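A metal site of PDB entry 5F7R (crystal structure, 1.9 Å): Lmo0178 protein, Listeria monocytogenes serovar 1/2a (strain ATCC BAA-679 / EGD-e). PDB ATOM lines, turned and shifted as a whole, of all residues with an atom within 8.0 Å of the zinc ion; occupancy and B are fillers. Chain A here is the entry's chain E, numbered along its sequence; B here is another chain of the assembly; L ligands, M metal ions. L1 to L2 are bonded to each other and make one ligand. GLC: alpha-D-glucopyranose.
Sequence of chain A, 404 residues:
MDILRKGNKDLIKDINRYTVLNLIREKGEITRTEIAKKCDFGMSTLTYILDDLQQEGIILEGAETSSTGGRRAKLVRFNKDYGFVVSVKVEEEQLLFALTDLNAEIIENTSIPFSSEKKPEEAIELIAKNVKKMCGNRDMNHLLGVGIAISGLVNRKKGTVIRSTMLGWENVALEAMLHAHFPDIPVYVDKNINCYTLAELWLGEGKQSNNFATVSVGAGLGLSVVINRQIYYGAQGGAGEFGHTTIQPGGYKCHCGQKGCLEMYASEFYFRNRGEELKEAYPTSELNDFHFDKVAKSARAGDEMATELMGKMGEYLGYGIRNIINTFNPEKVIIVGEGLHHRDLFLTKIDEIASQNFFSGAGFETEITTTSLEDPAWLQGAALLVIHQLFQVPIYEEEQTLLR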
ATOM      1  N   ARG A 163      36.516 -10.491   8.045  1.00  0.00           N
ATOM      2  CA  ARG A 163      35.611 -11.620   7.924  1.00  0.00           C
ATOM      3  C   ARG A 163      34.175 -11.113   7.768  1.00  0.00           C
ATOM      4  O   ARG A 163      33.580 -10.638   8.739  1.00  0.00           O
ATOM      5  CB  ARG A 163      35.704 -12.530   9.167  1.00  0.00           C
ATOM      6  CG  ARG A 163      34.886 -13.823   9.093  1.00  0.00           C
ATOM      7  CD  ARG A 163      34.889 -14.595  10.406  1.00  0.00           C
ATOM      8  NE  ARG A 163      34.371 -15.948  10.212  1.00  0.00           N
ATOM      9  CZ  ARG A 163      33.450 -16.562  10.947  1.00  0.00           C
ATOM     10  NH1 ARG A 163      33.013 -16.058  12.096  1.00  0.00           N
ATOM     11  NH2 ARG A 163      33.045 -17.770  10.576  1.00  0.00           N
ATOM     12  N   THR A 165      30.912 -13.080   6.796  1.00  0.00           N
ATOM     13  CA  THR A 165      30.243 -14.304   6.430  1.00  0.00           C
ATOM     14  C   THR A 165      28.968 -14.003   5.641  1.00  0.00           C
ATOM     15  O   THR A 165      28.451 -14.878   4.978  1.00  0.00           O
ATOM     16  CB  THR A 165      29.948 -15.160   7.649  1.00  0.00           C
ATOM     17  OG1 THR A 165      29.084 -14.446   8.540  1.00  0.00           O
ATOM     18  CG2 THR A 165      31.237 -15.507   8.343  1.00  0.00           C
ATOM     19  N   GLU A 241      28.159  -7.814  17.151  1.00  0.00           N
ATOM     20  CA  GLU A 241      27.711  -8.950  16.335  1.00  0.00           C
ATOM     21  C   GLU A 241      26.591  -9.690  17.009  1.00  0.00           C
ATOM     22  O   GLU A 241      26.601 -10.938  17.176  1.00  0.00           O
ATOM     23  CB  GLU A 241      28.848  -9.874  15.909  1.00  0.00           C
ATOM     24  CG  GLU A 241      29.769  -9.279  14.858  1.00  0.00           C
ATOM     25  CD  GLU A 241      29.086  -8.997  13.509  1.00  0.00           C
ATOM     26  OE1 GLU A 241      28.120  -9.693  13.101  1.00  0.00           O
ATOM     27  OE2 GLU A 241      29.530  -8.036  12.833  1.00  0.00           O
ATOM     28  N   PHE A 242      25.576  -8.911  17.321  1.00  0.00           N
ATOM     29  CA  PHE A 242      24.423  -9.380  18.025  1.00  0.00           C
ATOM     30  C   PHE A 242      23.598 -10.381  17.245  1.00  0.00           C
ATOM     31  O   PHE A 242      22.897 -11.213  17.825  1.00  0.00           O
ATOM     32  CB  PHE A 242      23.540  -8.205  18.400  1.00  0.00           C
ATOM     33  CG  PHE A 242      22.675  -8.484  19.573  1.00  0.00           C
ATOM     34  CD1 PHE A 242      23.271  -8.625  20.829  1.00  0.00           C
ATOM     35  CD2 PHE A 242      21.316  -8.677  19.432  1.00  0.00           C
ATOM     36  CE1 PHE A 242      22.513  -8.910  21.937  1.00  0.00           C
ATOM     37  CE2 PHE A 242      20.562  -8.999  20.544  1.00  0.00           C
ATOM     38  CZ  PHE A 242      21.150  -9.120  21.788  1.00  0.00           C
ATOM     39  N   GLY A 243      23.668 -10.294  15.923  1.00  0.00           N
ATOM     40  CA  GLY A 243      23.062 -11.290  15.049  1.00  0.00           C
ATOM     41  C   GLY A 243      23.572 -12.698  15.299  1.00  0.00           C
ATOM     42  O   GLY A 243      22.890 -13.681  14.966  1.00  0.00           O
ATOM     43  N   HIS A 244      24.770 -12.798  15.853  1.00  0.00           N
ATOM     44  CA  HIS A 244      25.394 -14.095  16.122  1.00  0.00           C
ATOM     45  C   HIS A 244      25.487 -14.406  17.592  1.00  0.00           C
ATOM     46  O   HIS A 244      26.331 -15.192  18.015  1.00  0.00           O
ATOM     47  CB  HIS A 244      26.739 -14.106  15.399  1.00  0.00           C
ATOM     48  CG  HIS A 244      26.578 -13.748  13.983  1.00  0.00           C
ATOM     49  ND1 HIS A 244      25.943 -14.603  13.097  1.00  0.00           N
ATOM     50  CD2 HIS A 244      26.640 -12.547  13.365  1.00  0.00           C
ATOM     51  CE1 HIS A 244      25.693 -13.948  11.974  1.00  0.00           C
ATOM     52  NE2 HIS A 244      26.174 -12.727  12.084  1.00  0.00           N
ATOM     53  N   THR A 245      24.592 -13.821  18.391  1.00  0.00           N
ATOM     54  CA  THR A 245      24.274 -14.363  19.686  1.00  0.00           C
ATOM     55  C   THR A 245      23.355 -15.552  19.508  1.00  0.00           C
ATOM     56  O   THR A 245      22.575 -15.604  18.554  1.00  0.00           O
ATOM     57  CB  THR A 245      23.619 -13.327  20.634  1.00  0.00           C
ATOM     58  OG1 THR A 245      22.424 -12.794  20.047  1.00  0.00           O
ATOM     59  CG2 THR A 245      24.587 -12.227  20.934  1.00  0.00           C
ATOM     60  N   THR A 246      23.466 -16.527  20.382  1.00  0.00           N
ATOM     61  CA  THR A 246      22.628 -17.727  20.274  1.00  0.00           C
ATOM     62  C   THR A 246      21.269 -17.467  20.903  1.00  0.00           C
ATOM     63  O   THR A 246      21.197 -17.151  22.077  1.00  0.00           O
ATOM     64  CB  THR A 246      23.293 -18.904  20.999  1.00  0.00           C
ATOM     65  OG1 THR A 246      24.611 -19.045  20.495  1.00  0.00           O
ATOM     66  CG2 THR A 246      22.505 -20.181  20.772  1.00  0.00           C
ATOM     67  N   TYR A 252      19.094 -23.347  13.825  1.00  0.00           N
ATOM     68  CA  TYR A 252      19.472 -23.287  12.424  1.00  0.00           C
ATOM     69  C   TYR A 252      20.972 -23.020  12.269  1.00  0.00           C
ATOM     70  O   TYR A 252      21.523 -22.123  12.914  1.00  0.00           O
ATOM     71  CB  TYR A 252      18.688 -22.208  11.681  1.00  0.00           C
ATOM     72  CG  TYR A 252      17.218 -22.503  11.526  1.00  0.00           C
ATOM     73  CD1 TYR A 252      16.782 -23.691  10.933  1.00  0.00           C
ATOM     74  CD2 TYR A 252      16.253 -21.621  12.012  1.00  0.00           C
ATOM     75  CE1 TYR A 252      15.429 -23.990  10.838  1.00  0.00           C
ATOM     76  CE2 TYR A 252      14.893 -21.899  11.881  1.00  0.00           C
ATOM     77  CZ  TYR A 252      14.495 -23.085  11.290  1.00  0.00           C
ATOM     78  OH  TYR A 252      13.142 -23.361  11.151  1.00  0.00           O
ATOM     79  N   LYS A 253      21.593 -23.724  11.344  1.00  0.00           N
ATOM     80  CA  LYS A 253      22.979 -23.466  10.973  1.00  0.00           C
ATOM     81  C   LYS A 253      23.105 -22.067  10.366  1.00  0.00           C
ATOM     82  O   LYS A 253      22.361 -21.748   9.461  1.00  0.00           O
ATOM     83  CB  LYS A 253      23.427 -24.507   9.936  1.00  0.00           C
ATOM     84  CG  LYS A 253      24.843 -24.334   9.404  1.00  0.00           C
ATOM     85  CD  LYS A 253      25.887 -24.670  10.460  1.00  0.00           C
ATOM     86  CE  LYS A 253      27.294 -24.624   9.841  1.00  0.00           C
ATOM     87  NZ  LYS A 253      28.300 -25.313  10.685  1.00  0.00           N
ATOM     88  N   CYS A 254      24.025 -21.253  10.882  1.00  0.00           N
ATOM     89  CA  CYS A 254      24.259 -19.901  10.377  1.00  0.00           C
ATOM     90  C   CYS A 254      25.434 -19.851   9.381  1.00  0.00           C
ATOM     91  O   CYS A 254      26.341 -20.666   9.454  1.00  0.00           O
ATOM     92  CB  CYS A 254      24.525 -18.958  11.561  1.00  0.00           C
ATOM     93  SG  CYS A 254      24.693 -17.187  11.174  1.00  0.00           S
ATOM     94  N   HIS A 255      25.460 -18.809   8.554  1.00  0.00           N
ATOM     95  CA  HIS A 255      26.609 -18.517   7.684  1.00  0.00           C
ATOM     96  C   HIS A 255      27.914 -18.294   8.453  1.00  0.00           C
ATOM     97  O   HIS A 255      29.006 -18.550   7.923  1.00  0.00           O
ATOM     98  CB  HIS A 255      26.322 -17.341   6.710  1.00  0.00           C
ATOM     99  CG  HIS A 255      25.745 -16.120   7.378  1.00  0.00           C
ATOM    100  ND1 HIS A 255      26.528 -15.182   7.989  1.00  0.00           N
ATOM    101  CD2 HIS A 255      24.467 -15.726   7.559  1.00  0.00           C
ATOM    102  CE1 HIS A 255      25.767 -14.233   8.494  1.00  0.00           C
ATOM    103  NE2 HIS A 255      24.510 -14.542   8.261  1.00  0.00           N
ATOM    104  N   CYS A 256      27.803 -17.920   9.733  1.00  0.00           N
ATOM    105  CA  CYS A 256      28.982 -17.722  10.568  1.00  0.00           C
ATOM    106  C   CYS A 256      29.597 -19.050  11.076  1.00  0.00           C
ATOM    107  O   CYS A 256      30.648 -19.029  11.692  1.00  0.00           O
ATOM    108  CB  CYS A 256      28.661 -16.759  11.711  1.00  0.00           C
ATOM    109  SG  CYS A 256      27.883 -17.544  13.164  1.00  0.00           S
ATOM    110  N   GLY A 257      28.957 -20.185  10.813  1.00  0.00           N
ATOM    111  CA  GLY A 257      29.425 -21.476  11.278  1.00  0.00           C
ATOM    112  C   GLY A 257      28.754 -21.988  12.555  1.00  0.00           C
ATOM    113  O   GLY A 257      28.730 -23.214  12.806  1.00  0.00           O
ATOM    114  N   GLN A 258      28.139 -21.087  13.344  1.00  0.00           N
ATOM    115  CA  GLN A 258      27.430 -21.468  14.612  1.00  0.00           C
ATOM    116  C   GLN A 258      26.029 -22.041  14.311  1.00  0.00           C
ATOM    117  O   GLN A 258      25.561 -21.938  13.176  1.00  0.00           O
ATOM    118  CB  GLN A 258      27.298 -20.257  15.566  1.00  0.00           C
ATOM    119  CG  GLN A 258      28.616 -19.575  15.919  1.00  0.00           C
ATOM    120  CD  GLN A 258      28.485 -18.245  16.670  1.00  0.00           C
ATOM    121  OE1 GLN A 258      29.491 -17.543  16.851  1.00  0.00           O
ATOM    122  NE2 GLN A 258      27.272 -17.903  17.139  1.00  0.00           N
ATOM    123  N   LYS A 259      25.385 -22.653  15.304  1.00  0.00           N
ATOM    124  CA  LYS A 259      23.974 -23.000  15.175  1.00  0.00           C
ATOM    125  C   LYS A 259      23.169 -22.107  16.092  1.00  0.00           C
ATOM    126  O   LYS A 259      23.611 -21.772  17.202  1.00  0.00           O
ATOM    127  CB  LYS A 259      23.774 -24.482  15.468  1.00  0.00           C
ATOM    128  CG  LYS A 259      24.247 -25.355  14.299  1.00  0.00           C
ATOM    129  CD  LYS A 259      24.204 -26.853  14.613  1.00  0.00           C
ATOM    130  CE  LYS A 259      22.783 -27.394  14.746  1.00  0.00           C
ATOM    131  NZ  LYS A 259      21.885 -27.124  13.569  1.00  0.00           N
ATOM    132  N   GLY A 260      21.985 -21.709  15.648  1.00  0.00           N
ATOM    133  CA  GLY A 260      21.019 -21.079  16.526  1.00  0.00           C
ATOM    134  C   GLY A 260      21.173 -19.570  16.710  1.00  0.00           C
ATOM    135  O   GLY A 260      20.613 -18.994  17.650  1.00  0.00           O
ATOM    136  N   CYS A 261      21.930 -18.932  15.836  1.00  0.00           N
ATOM    137  CA  CYS A 261      22.111 -17.495  15.900  1.00  0.00           C
ATOM    138  C   CYS A 261      20.792 -16.735  15.736  1.00  0.00           C
ATOM    139  O   CYS A 261      19.917 -17.117  14.949  1.00  0.00           O
ATOM    140  CB  CYS A 261      23.064 -17.039  14.812  1.00  0.00           C
ATOM    141  SG  CYS A 261      24.718 -17.675  14.996  1.00  0.00           S
ATOM    142  N   LEU A 262      20.686 -15.649  16.475  1.00  0.00           N
ATOM    143  CA  LEU A 262      19.540 -14.777  16.476  1.00  0.00           C
ATOM    144  C   LEU A 262      19.150 -14.358  15.055  1.00  0.00           C
ATOM    145  O   LEU A 262      17.965 -14.379  14.701  1.00  0.00           O
ATOM    146  CB  LEU A 262      19.862 -13.527  17.290  1.00  0.00           C
ATOM    147  CG  LEU A 262      18.746 -12.496  17.394  1.00  0.00           C
ATOM    148  CD1 LEU A 262      17.502 -13.127  17.988  1.00  0.00           C
ATOM    149  CD2 LEU A 262      19.232 -11.336  18.234  1.00  0.00           C
ATOM    150  N   GLU A 263      20.149 -14.094  14.220  1.00  0.00           N
ATOM    151  CA  GLU A 263      19.932 -13.700  12.828  1.00  0.00           C
ATOM    152  C   GLU A 263      19.232 -14.776  11.999  1.00  0.00           C
ATOM    153  O   GLU A 263      18.597 -14.485  10.984  1.00  0.00           O
ATOM    154  CB  GLU A 263      21.296 -13.356  12.238  1.00  0.00           C
ATOM    155  CG  GLU A 263      21.336 -12.949  10.807  1.00  0.00           C
ATOM    156  CD  GLU A 263      22.587 -12.157  10.542  1.00  0.00           C
ATOM    157  OE1 GLU A 263      23.476 -12.716   9.851  1.00  0.00           O
ATOM    158  OE2 GLU A 263      22.717 -11.065  11.135  1.00  0.00           O
ATOM    159  N   MET A 264      19.335 -16.034  12.424  1.00  0.00           N
ATOM    160  CA  MET A 264      18.652 -17.112  11.723  1.00  0.00           C
ATOM    161  C   MET A 264      17.157 -17.123  12.007  1.00  0.00           C
ATOM    162  O   MET A 264      16.431 -17.865  11.350  1.00  0.00           O
ATOM    163  CB  MET A 264      19.304 -18.467  12.044  1.00  0.00           C
ATOM    164  CG  MET A 264      20.740 -18.602  11.514  1.00  0.00           C
ATOM    165  SD  MET A 264      20.905 -18.422   9.725  1.00  0.00           S
ATOM    166  CE  MET A 264      21.370 -16.701   9.554  1.00  0.00           C
ATOM    167  N   ARG B 322      29.784 -16.996  24.941  1.00  0.00           N
ATOM    168  CA  ARG B 322      29.827 -16.726  23.505  1.00  0.00           C
ATOM    169  C   ARG B 322      29.062 -15.474  23.169  1.00  0.00           C
ATOM    170  O   ARG B 322      29.551 -14.616  22.403  1.00  0.00           O
ATOM    171  CB  ARG B 322      29.297 -17.905  22.678  1.00  0.00           C
ATOM    172  CG  ARG B 322      29.293 -17.632  21.170  1.00  0.00           C
ATOM    173  CD  ARG B 322      28.410 -18.636  20.424  1.00  0.00           C
ATOM    174  NE  ARG B 322      29.068 -19.922  20.412  1.00  0.00           N
ATOM    175  CZ  ARG B 322      28.552 -21.038  19.899  1.00  0.00           C
ATOM    176  NH1 ARG B 322      29.260 -22.156  19.942  1.00  0.00           N
ATOM    177  NH2 ARG B 322      27.333 -21.057  19.405  1.00  0.00           N
ATOM    178  N   ASN B 326      30.575 -12.037  21.362  1.00  0.00           N
ATOM    179  CA  ASN B 326      30.075 -11.507  20.090  1.00  0.00           C
ATOM    180  C   ASN B 326      29.434 -10.152  20.228  1.00  0.00           C
ATOM    181  O   ASN B 326      29.490  -9.336  19.308  1.00  0.00           O
ATOM    182  CB  ASN B 326      29.108 -12.494  19.442  1.00  0.00           C
ATOM    183  CG  ASN B 326      29.801 -13.711  18.887  1.00  0.00           C
ATOM    184  OD1 ASN B 326      31.042 -13.760  18.795  1.00  0.00           O
ATOM    185  ND2 ASN B 326      29.012 -14.709  18.457  1.00  0.00           N
ATOM    186  N   PHE B 358      32.535 -15.234  16.863  1.00  0.00           N
ATOM    187  CA  PHE B 358      32.593 -14.590  15.565  1.00  0.00           C
ATOM    188  C   PHE B 358      34.033 -14.223  15.180  1.00  0.00           C
ATOM    189  O   PHE B 358      34.395 -14.311  14.027  1.00  0.00           O
ATOM    190  CB  PHE B 358      31.704 -13.357  15.504  1.00  0.00           C
ATOM    191  CG  PHE B 358      31.448 -12.887  14.096  1.00  0.00           C
ATOM    192  CD1 PHE B 358      30.457 -13.466  13.323  1.00  0.00           C
ATOM    193  CD2 PHE B 358      32.284 -11.957  13.506  1.00  0.00           C
ATOM    194  CE1 PHE B 358      30.257 -13.081  12.005  1.00  0.00           C
ATOM    195  CE2 PHE B 358      32.094 -11.551  12.189  1.00  0.00           C
ATOM    196  CZ  PHE B 358      31.066 -12.108  11.436  1.00  0.00           C
HETATM  197  C1  GLC L   1      25.338  -9.597   9.843  1.00  0.00           C
HETATM  198  C2  GLC L   1      26.783  -9.110   9.889  1.00  0.00           C
HETATM  199  C3  GLC L   1      26.883  -7.810  10.672  1.00  0.00           C
HETATM  200  C4  GLC L   1      25.941  -6.772  10.082  1.00  0.00           C
HETATM  201  C5  GLC L   1      24.527  -7.353  10.091  1.00  0.00           C
HETATM  202  C6  GLC L   1      23.486  -6.391   9.582  1.00  0.00           C
HETATM  203  O1  GLC L   1      24.958  -9.959  11.179  1.00  0.00           O
HETATM  204  O2  GLC L   1      27.620 -10.087  10.525  1.00  0.00           O
HETATM  205  O3  GLC L   1      28.259  -7.384  10.647  1.00  0.00           O
HETATM  206  O4  GLC L   1      25.932  -5.550  10.847  1.00  0.00           O
HETATM  207  O5  GLC L   1      24.490  -8.557   9.336  1.00  0.00           O
HETATM  208  O6  GLC L   1      23.739  -6.076   8.201  1.00  0.00           O
HETATM  209  C1  GLC L   2      22.843  -6.767   7.306  1.00  0.00           C
HETATM  210  C2  GLC L   2      23.170  -6.380   5.862  1.00  0.00           C
HETATM  211  C3  GLC L   2      22.812  -4.927   5.586  1.00  0.00           C
HETATM  212  C4  GLC L   2      21.360  -4.689   5.972  1.00  0.00           C
HETATM  213  C5  GLC L   2      21.125  -5.113   7.420  1.00  0.00           C
HETATM  214  C6  GLC L   2      19.690  -4.914   7.895  1.00  0.00           C
HETATM  215  O2  GLC L   2      24.551  -6.605   5.595  1.00  0.00           O
HETATM  216  O3  GLC L   2      23.067  -4.588   4.201  1.00  0.00           O
HETATM  217  O4  GLC L   2      21.025  -3.298   5.846  1.00  0.00           O
HETATM  218  O5  GLC L   2      21.476  -6.489   7.576  1.00  0.00           O
HETATM  219  O6  GLC L   2      19.568  -5.256   9.287  1.00  0.00           O
HETATM  220 ZN    ZN M   1      25.777 -16.676  13.177  1.00  0.00          ZN
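NE2 of His 244 lies within hydrogen-bond range of O1 of GLC L1 (3.2 Å).
The side-chain carboxylate of Glu 263 lies within hydrogen-bond range of an oxygen (O1) of GLC L1, at 2.5 Å.
O3 of GLC L1 sits at hydrogen-bond distance from OE2 of Glu 241 (2.6 Å).
The backbone carbonyl oxygen (O) of His 244 lies within hydrogen-bond range of the side-chain amide nitrogen (NE2) of Gln 258 (3.0 Å).
ND2 of Asn 326 of chain B is in hydrogen-bond range of O of His 244 (2.8 Å).
SG of Cys 256 lies close to N of Gln 258 (3.6 Å).
O of Cys 256 is in hydrogen-bond range of NH2 of Arg 163, 2.9 Å away.
SG of Cys 261 lies close to NE2 of Gln 258 (3.3 Å).
Four residues have an atom within 4 Å of the zinc ion: His 244, Cys 254, Cys 256 and Cys 261.
The zinc ion is bound by a ring nitrogen (ND1) of His 244, at 2.1 Å.
The side-chain sulfur (SG) of Cys 256 binds the zinc ion (2.3 Å).
SG of Cys 261 binds the zinc ion.
The zinc ion is bound by SG of Cys 254, 2.3 Å away.
The zinc ion has four donor atoms within binding distance.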
